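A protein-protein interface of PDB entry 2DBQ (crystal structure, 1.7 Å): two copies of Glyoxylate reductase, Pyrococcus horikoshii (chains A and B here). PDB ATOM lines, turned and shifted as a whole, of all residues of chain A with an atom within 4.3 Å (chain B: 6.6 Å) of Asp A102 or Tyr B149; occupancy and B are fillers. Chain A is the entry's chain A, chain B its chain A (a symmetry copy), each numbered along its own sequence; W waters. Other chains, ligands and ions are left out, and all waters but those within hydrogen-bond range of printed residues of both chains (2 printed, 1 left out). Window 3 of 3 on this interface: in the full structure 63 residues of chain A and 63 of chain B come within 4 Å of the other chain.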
ATOM      1  N   LEU A 100       4.663  19.680  -2.002  1.00  0.00           N
ATOM      2  CA  LEU A 100       4.955  19.771  -3.431  1.00  0.00           C
ATOM      3  C   LEU A 100       5.765  18.563  -3.919  1.00  0.00           C
ATOM      4  O   LEU A 100       6.204  18.523  -5.071  1.00  0.00           O
ATOM      5  CB  LEU A 100       5.731  21.063  -3.732  1.00  0.00           C
ATOM      6  CG  LEU A 100       6.896  21.479  -2.821  1.00  0.00           C
ATOM      7  CD1 LEU A 100       7.920  20.353  -2.690  1.00  0.00           C
ATOM      8  CD2 LEU A 100       7.549  22.726  -3.396  1.00  0.00           C
ATOM      9  N   THR A 101       5.955  17.577  -3.044  1.00  0.00           N
ATOM     10  CA  THR A 101       6.736  16.395  -3.400  1.00  0.00           C
ATOM     11  C   THR A 101       6.189  15.612  -4.586  1.00  0.00           C
ATOM     12  O   THR A 101       6.925  15.296  -5.521  1.00  0.00           O
ATOM     13  CB  THR A 101       6.862  15.426  -2.210  1.00  0.00           C
ATOM     14  OG1 THR A 101       7.636  16.046  -1.183  1.00  0.00           O
ATOM     15  CG2 THR A 101       7.547  14.125  -2.641  1.00  0.00           C
ATOM     16  N   ASP A 102       4.900  15.301  -4.558  1.00  0.00           N
ATOM     17  CA  ASP A 102       4.328  14.524  -5.646  1.00  0.00           C
ATOM     18  C   ASP A 102       4.214  15.267  -6.965  1.00  0.00           C
ATOM     19  O   ASP A 102       4.319  14.650  -8.024  1.00  0.00           O
ATOM     20  CB  ASP A 102       2.985  13.945  -5.222  1.00  0.00           C
ATOM     21  CG  ASP A 102       3.141  12.908  -4.130  1.00  0.00           C
ATOM     22  OD1 ASP A 102       3.987  12.002  -4.303  1.00  0.00           O
ATOM     23  OD2 ASP A 102       2.435  12.998  -3.107  1.00  0.00           O
ATOM     24  N   ALA A 103       4.020  16.583  -6.918  1.00  0.00           N
ATOM     25  CA  ALA A 103       3.937  17.351  -8.158  1.00  0.00           C
ATOM     26  C   ALA A 103       5.312  17.366  -8.835  1.00  0.00           C
ATOM     27  O   ALA A 103       5.422  17.159 -10.044  1.00  0.00           O
ATOM     28  CB  ALA A 103       3.477  18.779  -7.874  1.00  0.00           C
ATOM     29  N   THR A 104       6.360  17.586  -8.046  1.00  0.00           N
ATOM     30  CA  THR A 104       7.712  17.645  -8.586  1.00  0.00           C
ATOM     31  C   THR A 104       8.188  16.276  -9.075  1.00  0.00           C
ATOM     32  O   THR A 104       8.852  16.178 -10.109  1.00  0.00           O
ATOM     33  CB  THR A 104       8.704  18.197  -7.537  1.00  0.00           C
ATOM     34  OG1 THR A 104       8.163  19.389  -6.957  1.00  0.00           O
ATOM     35  CG2 THR A 104      10.040  18.542  -8.190  1.00  0.00           C
ATOM     36  N   ALA A 105       7.847  15.221  -8.337  1.00  0.00           N
ATOM     37  CA  ALA A 105       8.238  13.868  -8.735  1.00  0.00           C
ATOM     38  C   ALA A 105       7.500  13.507 -10.023  1.00  0.00           C
ATOM     39  O   ALA A 105       8.054  12.833 -10.890  1.00  0.00           O
ATOM     40  CB  ALA A 105       7.908  12.871  -7.632  1.00  0.00           C
ATOM     41  N   ASP A 106       6.251  13.958 -10.147  1.00  0.00           N
ATOM     42  CA  ASP A 106       5.458  13.704 -11.353  1.00  0.00           C
ATOM     43  C   ASP A 106       6.124  14.406 -12.534  1.00  0.00           C
ATOM     44  O   ASP A 106       6.296  13.815 -13.602  1.00  0.00           O
ATOM     45  CB  ASP A 106       4.028  14.244 -11.211  1.00  0.00           C
ATOM     46  CG  ASP A 106       3.127  13.348 -10.369  1.00  0.00           C
ATOM     47  OD1 ASP A 106       3.594  12.291  -9.892  1.00  0.00           O
ATOM     48  OD2 ASP A 106       1.937  13.711 -10.190  1.00  0.00           O
ATOM     49  N   ARG A 168       7.971   5.893  -8.058  1.00  0.00           N
ATOM     50  CA  ARG A 168       7.412   5.855  -9.403  1.00  0.00           C
ATOM     51  C   ARG A 168       8.251   4.924 -10.279  1.00  0.00           C
ATOM     52  O   ARG A 168       7.713   4.210 -11.124  1.00  0.00           O
ATOM     53  CB  ARG A 168       7.375   7.268  -9.996  1.00  0.00           C
ATOM     54  CG  ARG A 168       6.344   8.168  -9.317  1.00  0.00           C
ATOM     55  CD  ARG A 168       6.678   9.646  -9.483  1.00  0.00           C
ATOM     56  NE  ARG A 168       5.644  10.526  -8.926  1.00  0.00           N
ATOM     57  CZ  ARG A 168       5.323  10.616  -7.636  1.00  0.00           C
ATOM     58  NH1 ARG A 168       5.941   9.875  -6.721  1.00  0.00           N
ATOM     59  NH2 ARG A 168       4.389  11.478  -7.254  1.00  0.00           N
ATOM     60  N   ARG B 117       0.762  18.224 -17.332  1.00  0.00           N
ATOM     61  CA  ARG B 117       1.653  19.270 -16.844  1.00  0.00           C
ATOM     62  C   ARG B 117       2.147  20.318 -17.835  1.00  0.00           C
ATOM     63  O   ARG B 117       3.047  21.095 -17.520  1.00  0.00           O
ATOM     64  CB  ARG B 117       2.834  18.612 -16.122  1.00  0.00           C
ATOM     65  CG  ARG B 117       2.389  17.755 -14.924  1.00  0.00           C
ATOM     66  CD  ARG B 117       1.685  18.604 -13.867  1.00  0.00           C
ATOM     67  NE  ARG B 117       2.623  19.559 -13.293  1.00  0.00           N
ATOM     68  CZ  ARG B 117       3.459  19.282 -12.298  1.00  0.00           C
ATOM     69  NH1 ARG B 117       3.462  18.076 -11.745  1.00  0.00           N
ATOM     70  NH2 ARG B 117       4.323  20.201 -11.887  1.00  0.00           N
ATOM     71  N   TYR B 146      -2.416  19.358 -13.713  1.00  0.00           N
ATOM     72  CA  TYR B 146      -3.059  18.364 -12.872  1.00  0.00           C
ATOM     73  C   TYR B 146      -2.145  17.358 -12.206  1.00  0.00           C
ATOM     74  O   TYR B 146      -1.180  16.868 -12.796  1.00  0.00           O
ATOM     75  CB  TYR B 146      -4.116  17.617 -13.684  1.00  0.00           C
ATOM     76  CG  TYR B 146      -5.262  18.509 -14.081  1.00  0.00           C
ATOM     77  CD1 TYR B 146      -6.216  18.909 -13.139  1.00  0.00           C
ATOM     78  CD2 TYR B 146      -5.348  19.027 -15.372  1.00  0.00           C
ATOM     79  CE1 TYR B 146      -7.226  19.813 -13.473  1.00  0.00           C
ATOM     80  CE2 TYR B 146      -6.351  19.931 -15.717  1.00  0.00           C
ATOM     81  CZ  TYR B 146      -7.283  20.321 -14.762  1.00  0.00           C
ATOM     82  OH  TYR B 146      -8.253  21.233 -15.102  1.00  0.00           O
ATOM     83  N   ASP B 147      -2.462  17.064 -10.954  1.00  0.00           N
ATOM     84  CA  ASP B 147      -1.709  16.080 -10.204  1.00  0.00           C
ATOM     85  C   ASP B 147      -2.053  14.734 -10.823  1.00  0.00           C
ATOM     86  O   ASP B 147      -3.151  14.546 -11.353  1.00  0.00           O
ATOM     87  CB  ASP B 147      -2.132  16.096  -8.737  1.00  0.00           C
ATOM     88  CG  ASP B 147      -1.680  17.343  -8.027  1.00  0.00           C
ATOM     89  OD1 ASP B 147      -0.455  17.517  -7.880  1.00  0.00           O
ATOM     90  OD2 ASP B 147      -2.544  18.152  -7.627  1.00  0.00           O
ATOM     91  N   VAL B 148      -1.104  13.808 -10.777  1.00  0.00           N
ATOM     92  CA  VAL B 148      -1.322  12.474 -11.313  1.00  0.00           C
ATOM     93  C   VAL B 148      -1.298  11.495 -10.147  1.00  0.00           C
ATOM     94  O   VAL B 148      -2.170  10.635 -10.028  1.00  0.00           O
ATOM     95  CB  VAL B 148      -0.231  12.086 -12.338  1.00  0.00           C
ATOM     96  CG1 VAL B 148      -0.394  10.622 -12.752  1.00  0.00           C
ATOM     97  CG2 VAL B 148      -0.331  12.990 -13.558  1.00  0.00           C
ATOM     98  N   TYR B 149      -0.308  11.649  -9.276  1.00  0.00           N
ATOM     99  CA  TYR B 149      -0.165  10.779  -8.117  1.00  0.00           C
ATOM    100  C   TYR B 149      -1.441  10.758  -7.282  1.00  0.00           C
ATOM    101  O   TYR B 149      -2.002  11.804  -6.970  1.00  0.00           O
ATOM    102  CB  TYR B 149       1.008  11.252  -7.252  1.00  0.00           C
ATOM    103  CG  TYR B 149       1.488  10.235  -6.231  1.00  0.00           C
ATOM    104  CD1 TYR B 149       0.953  10.195  -4.940  1.00  0.00           C
ATOM    105  CD2 TYR B 149       2.475   9.306  -6.566  1.00  0.00           C
ATOM    106  CE1 TYR B 149       1.401   9.244  -4.002  1.00  0.00           C
ATOM    107  CE2 TYR B 149       2.927   8.358  -5.645  1.00  0.00           C
ATOM    108  CZ  TYR B 149       2.389   8.330  -4.367  1.00  0.00           C
ATOM    109  OH  TYR B 149       2.847   7.381  -3.473  1.00  0.00           O
ATOM    110  N   GLY B 150      -1.906   9.559  -6.941  1.00  0.00           N
ATOM    111  CA  GLY B 150      -3.100   9.433  -6.129  1.00  0.00           C
ATOM    112  C   GLY B 150      -4.414   9.691  -6.839  1.00  0.00           C
ATOM    113  O   GLY B 150      -5.478   9.512  -6.245  1.00  0.00           O
ATOM    114  N   LYS B 151      -4.355  10.102  -8.104  1.00  0.00           N
ATOM    115  CA  LYS B 151      -5.573  10.377  -8.858  1.00  0.00           C
ATOM    116  C   LYS B 151      -6.177   9.104  -9.452  1.00  0.00           C
ATOM    117  O   LYS B 151      -5.607   8.017  -9.335  1.00  0.00           O
ATOM    118  CB  LYS B 151      -5.294  11.410  -9.955  1.00  0.00           C
ATOM    119  CG  LYS B 151      -4.891  12.787  -9.412  1.00  0.00           C
ATOM    120  CD  LYS B 151      -5.993  13.395  -8.544  1.00  0.00           C
ATOM    121  CE  LYS B 151      -5.565  14.744  -7.979  1.00  0.00           C
ATOM    122  NZ  LYS B 151      -6.620  15.394  -7.155  1.00  0.00           N
ATOM    123  N   LYS B 170       0.295   2.090 -10.651  1.00  0.00           N
ATOM    124  CA  LYS B 170       0.456   1.735  -9.247  1.00  0.00           C
ATOM    125  C   LYS B 170       1.687   2.436  -8.676  1.00  0.00           C
ATOM    126  O   LYS B 170       1.757   2.711  -7.479  1.00  0.00           O
ATOM    127  CB  LYS B 170       0.570   0.215  -9.073  1.00  0.00           C
ATOM    128  CG  LYS B 170      -0.351  -0.316  -7.972  1.00  0.00           C
ATOM    129  CD  LYS B 170      -0.265  -1.826  -7.799  1.00  0.00           C
ATOM    130  CE  LYS B 170       0.996  -2.248  -7.061  1.00  0.00           C
ATOM    131  NZ  LYS B 170       1.030  -3.725  -6.863  1.00  0.00           N
ATOM    132  N   GLY B 171       2.649   2.735  -9.543  1.00  0.00           N
ATOM    133  CA  GLY B 171       3.845   3.436  -9.111  1.00  0.00           C
ATOM    134  C   GLY B 171       3.486   4.862  -8.722  1.00  0.00           C
ATOM    135  O   GLY B 171       4.215   5.517  -7.974  1.00  0.00           O
ATOM    136  N   PHE B 172       2.358   5.343  -9.242  1.00  0.00           N
ATOM    137  CA  PHE B 172       1.867   6.688  -8.946  1.00  0.00           C
ATOM    138  C   PHE B 172       0.731   6.629  -7.923  1.00  0.00           C
ATOM    139  O   PHE B 172       0.003   7.603  -7.732  1.00  0.00           O
ATOM    140  CB  PHE B 172       1.374   7.384 -10.223  1.00  0.00           C
ATOM    141  CG  PHE B 172       2.483   7.864 -11.116  1.00  0.00           C
ATOM    142  CD1 PHE B 172       3.215   6.962 -11.886  1.00  0.00           C
ATOM    143  CD2 PHE B 172       2.822   9.219 -11.161  1.00  0.00           C
ATOM    144  CE1 PHE B 172       4.272   7.400 -12.687  1.00  0.00           C
ATOM    145  CE2 PHE B 172       3.879   9.669 -11.959  1.00  0.00           C
ATOM    146  CZ  PHE B 172       4.606   8.759 -12.723  1.00  0.00           C
ATOM    147  N   ASN B 173       0.584   5.470  -7.285  1.00  0.00           N
ATOM    148  CA  ASN B 173      -0.429   5.253  -6.254  1.00  0.00           C
ATOM    149  C   ASN B 173      -1.823   5.693  -6.693  1.00  0.00           C
ATOM    150  O   ASN B 173      -2.579   6.279  -5.916  1.00  0.00           O
ATOM    151  CB  ASN B 173      -0.012   6.003  -4.987  1.00  0.00           C
ATOM    152  CG  ASN B 173      -0.842   5.624  -3.785  1.00  0.00           C
ATOM    153  OD1 ASN B 173      -1.091   4.444  -3.541  1.00  0.00           O
ATOM    154  ND2 ASN B 173      -1.266   6.623  -3.016  1.00  0.00           N
ATOM    155  N   MET B 174      -2.167   5.393  -7.939  1.00  0.00           N
ATOM    156  CA  MET B 174      -3.456   5.794  -8.471  1.00  0.00           C
ATOM    157  C   MET B 174      -4.576   4.809  -8.163  1.00  0.00           C
ATOM    158  O   MET B 174      -4.327   3.638  -7.855  1.00  0.00           O
ATOM    159  CB  MET B 174      -3.351   5.976  -9.987  1.00  0.00           C
ATOM    160  CG  MET B 174      -2.281   6.965 -10.419  1.00  0.00           C
ATOM    161  SD  MET B 174      -2.208   7.215 -12.352  1.00  0.00           S
ATOM    162  CE  MET B 174      -3.489   8.652 -12.522  1.00  0.00           C
ATOM    163  N   PHE B 207      -8.182  10.642 -15.485  1.00  0.00           N
ATOM    164  CA  PHE B 207      -7.425  10.347 -16.702  1.00  0.00           C
ATOM    165  C   PHE B 207      -8.063   9.131 -17.368  1.00  0.00           C
ATOM    166  O   PHE B 207      -8.190   8.076 -16.745  1.00  0.00           O
ATOM    167  CB  PHE B 207      -5.968  10.029 -16.364  1.00  0.00           C
ATOM    168  CG  PHE B 207      -5.239  11.168 -15.721  1.00  0.00           C
ATOM    169  CD1 PHE B 207      -4.719  12.205 -16.494  1.00  0.00           C
ATOM    170  CD2 PHE B 207      -5.126  11.240 -14.332  1.00  0.00           C
ATOM    171  CE1 PHE B 207      -4.102  13.303 -15.893  1.00  0.00           C
ATOM    172  CE2 PHE B 207      -4.511  12.333 -13.724  1.00  0.00           C
ATOM    173  CZ  PHE B 207      -3.999  13.366 -14.507  1.00  0.00           C
HETATM  174  O   HOH W   1       1.456  16.032 -11.818  1.00  0.00           O
HETATM  175  O   HOH W   2       5.481   9.572  -3.839  1.00  0.00           O
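The backbone carbonyl oxygen (O) of Ala A103 lies within hydrogen-bond range of the guanidinium group (NH1) of Arg B117 (2.8 Å). OD2 of Asp A106 lies within hydrogen-bond range of N of Val B148 (3.1 Å). N of Tyr B149 lies within hydrogen-bond range of OD2 of Asp A106 (3.2 Å).
The side-chain carboxylate (OD1) of Asp A102 is in salt-bridge range of the guanidinium group (NH2) of Arg A168. The side-chain carboxylate of Asp A106 is in salt-bridge range of the guanidinium group of Arg A168, at 2.9 Å. The backbone carbonyl oxygen of Phe B172 lies within hydrogen-bond range of the backbone NH of Gly B150, 2.8 Å away.
Among the printed residues, merely in contact across the chains: Arg A168 with Tyr B149, Asp A106 with Phe B172, Arg A168 with Gly B171, Asp A102 with Tyr B149, Arg A168 with Phe B172 and Asp A106 with Arg B117.
Asp A102 touches just one residue of chain B: Tyr B149 (3.6 Å). Of chain A, only Asp A102 (3.6 Å), Asp A106 (3.2 Å) and Arg A168 (3.0 Å) come within 4 Å of Tyr B149. Of the printed residues of chain A, Arg B117 touches Ala A103 (2.8 Å) and Asp A106 (3.9 Å). Printed residues of chain B within 4 Å of Ala A103: Arg B117 (2.8 Å). Of the printed residues of chain B, Arg A168 touches Tyr B149 (3.0 Å), Gly B171 (3.5 Å) and Phe B172 (3.6 Å). Printed residues of chain B within 4 Å of Asp A106: Arg B117 (3.9 Å), Val B148 (3.1 Å), Tyr B149 (3.2 Å) and Phe B172 (3.4 Å). Phe B207 touches none of the printed residues of chain A. Lys B151 touches none of the printed residues of chain A. The nearest residue of chain B that does not touch Asp A102 is Arg B117 (5.1 Å). The nearest printed residue of chain A that does not touch Arg B117 is Thr A104 (4.7 Å).
Of the 8 printed residues of chain A, 4 touch a printed residue of chain B. Printed residues of chain A that touch a printed residue of chain B: Asp A102, Ala A103, Asp A106 and Arg A168. Hydrophobic or aromatic side chains of chain A within 4 Å of the printed part of chain B: Ala A103. Of the 13 printed residues of chain B, 5 touch a printed residue of chain A.
No position is printed for both chains.
Water W1 lies within hydrogen-bond range of the guanidinium group of Arg B117, the side-chain carboxylate of Asp A106 and the backbone carbonyl oxygen of Tyr B146. Water W2 lies within hydrogen-bond range of the side-chain carboxylate (OD1) of Asp A102 (2.9 Å), the guanidinium group (NH1) of Arg A168 (2.9 Å) and the side-chain hydroxyl (OH) of Tyr B149 (3.4 Å).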
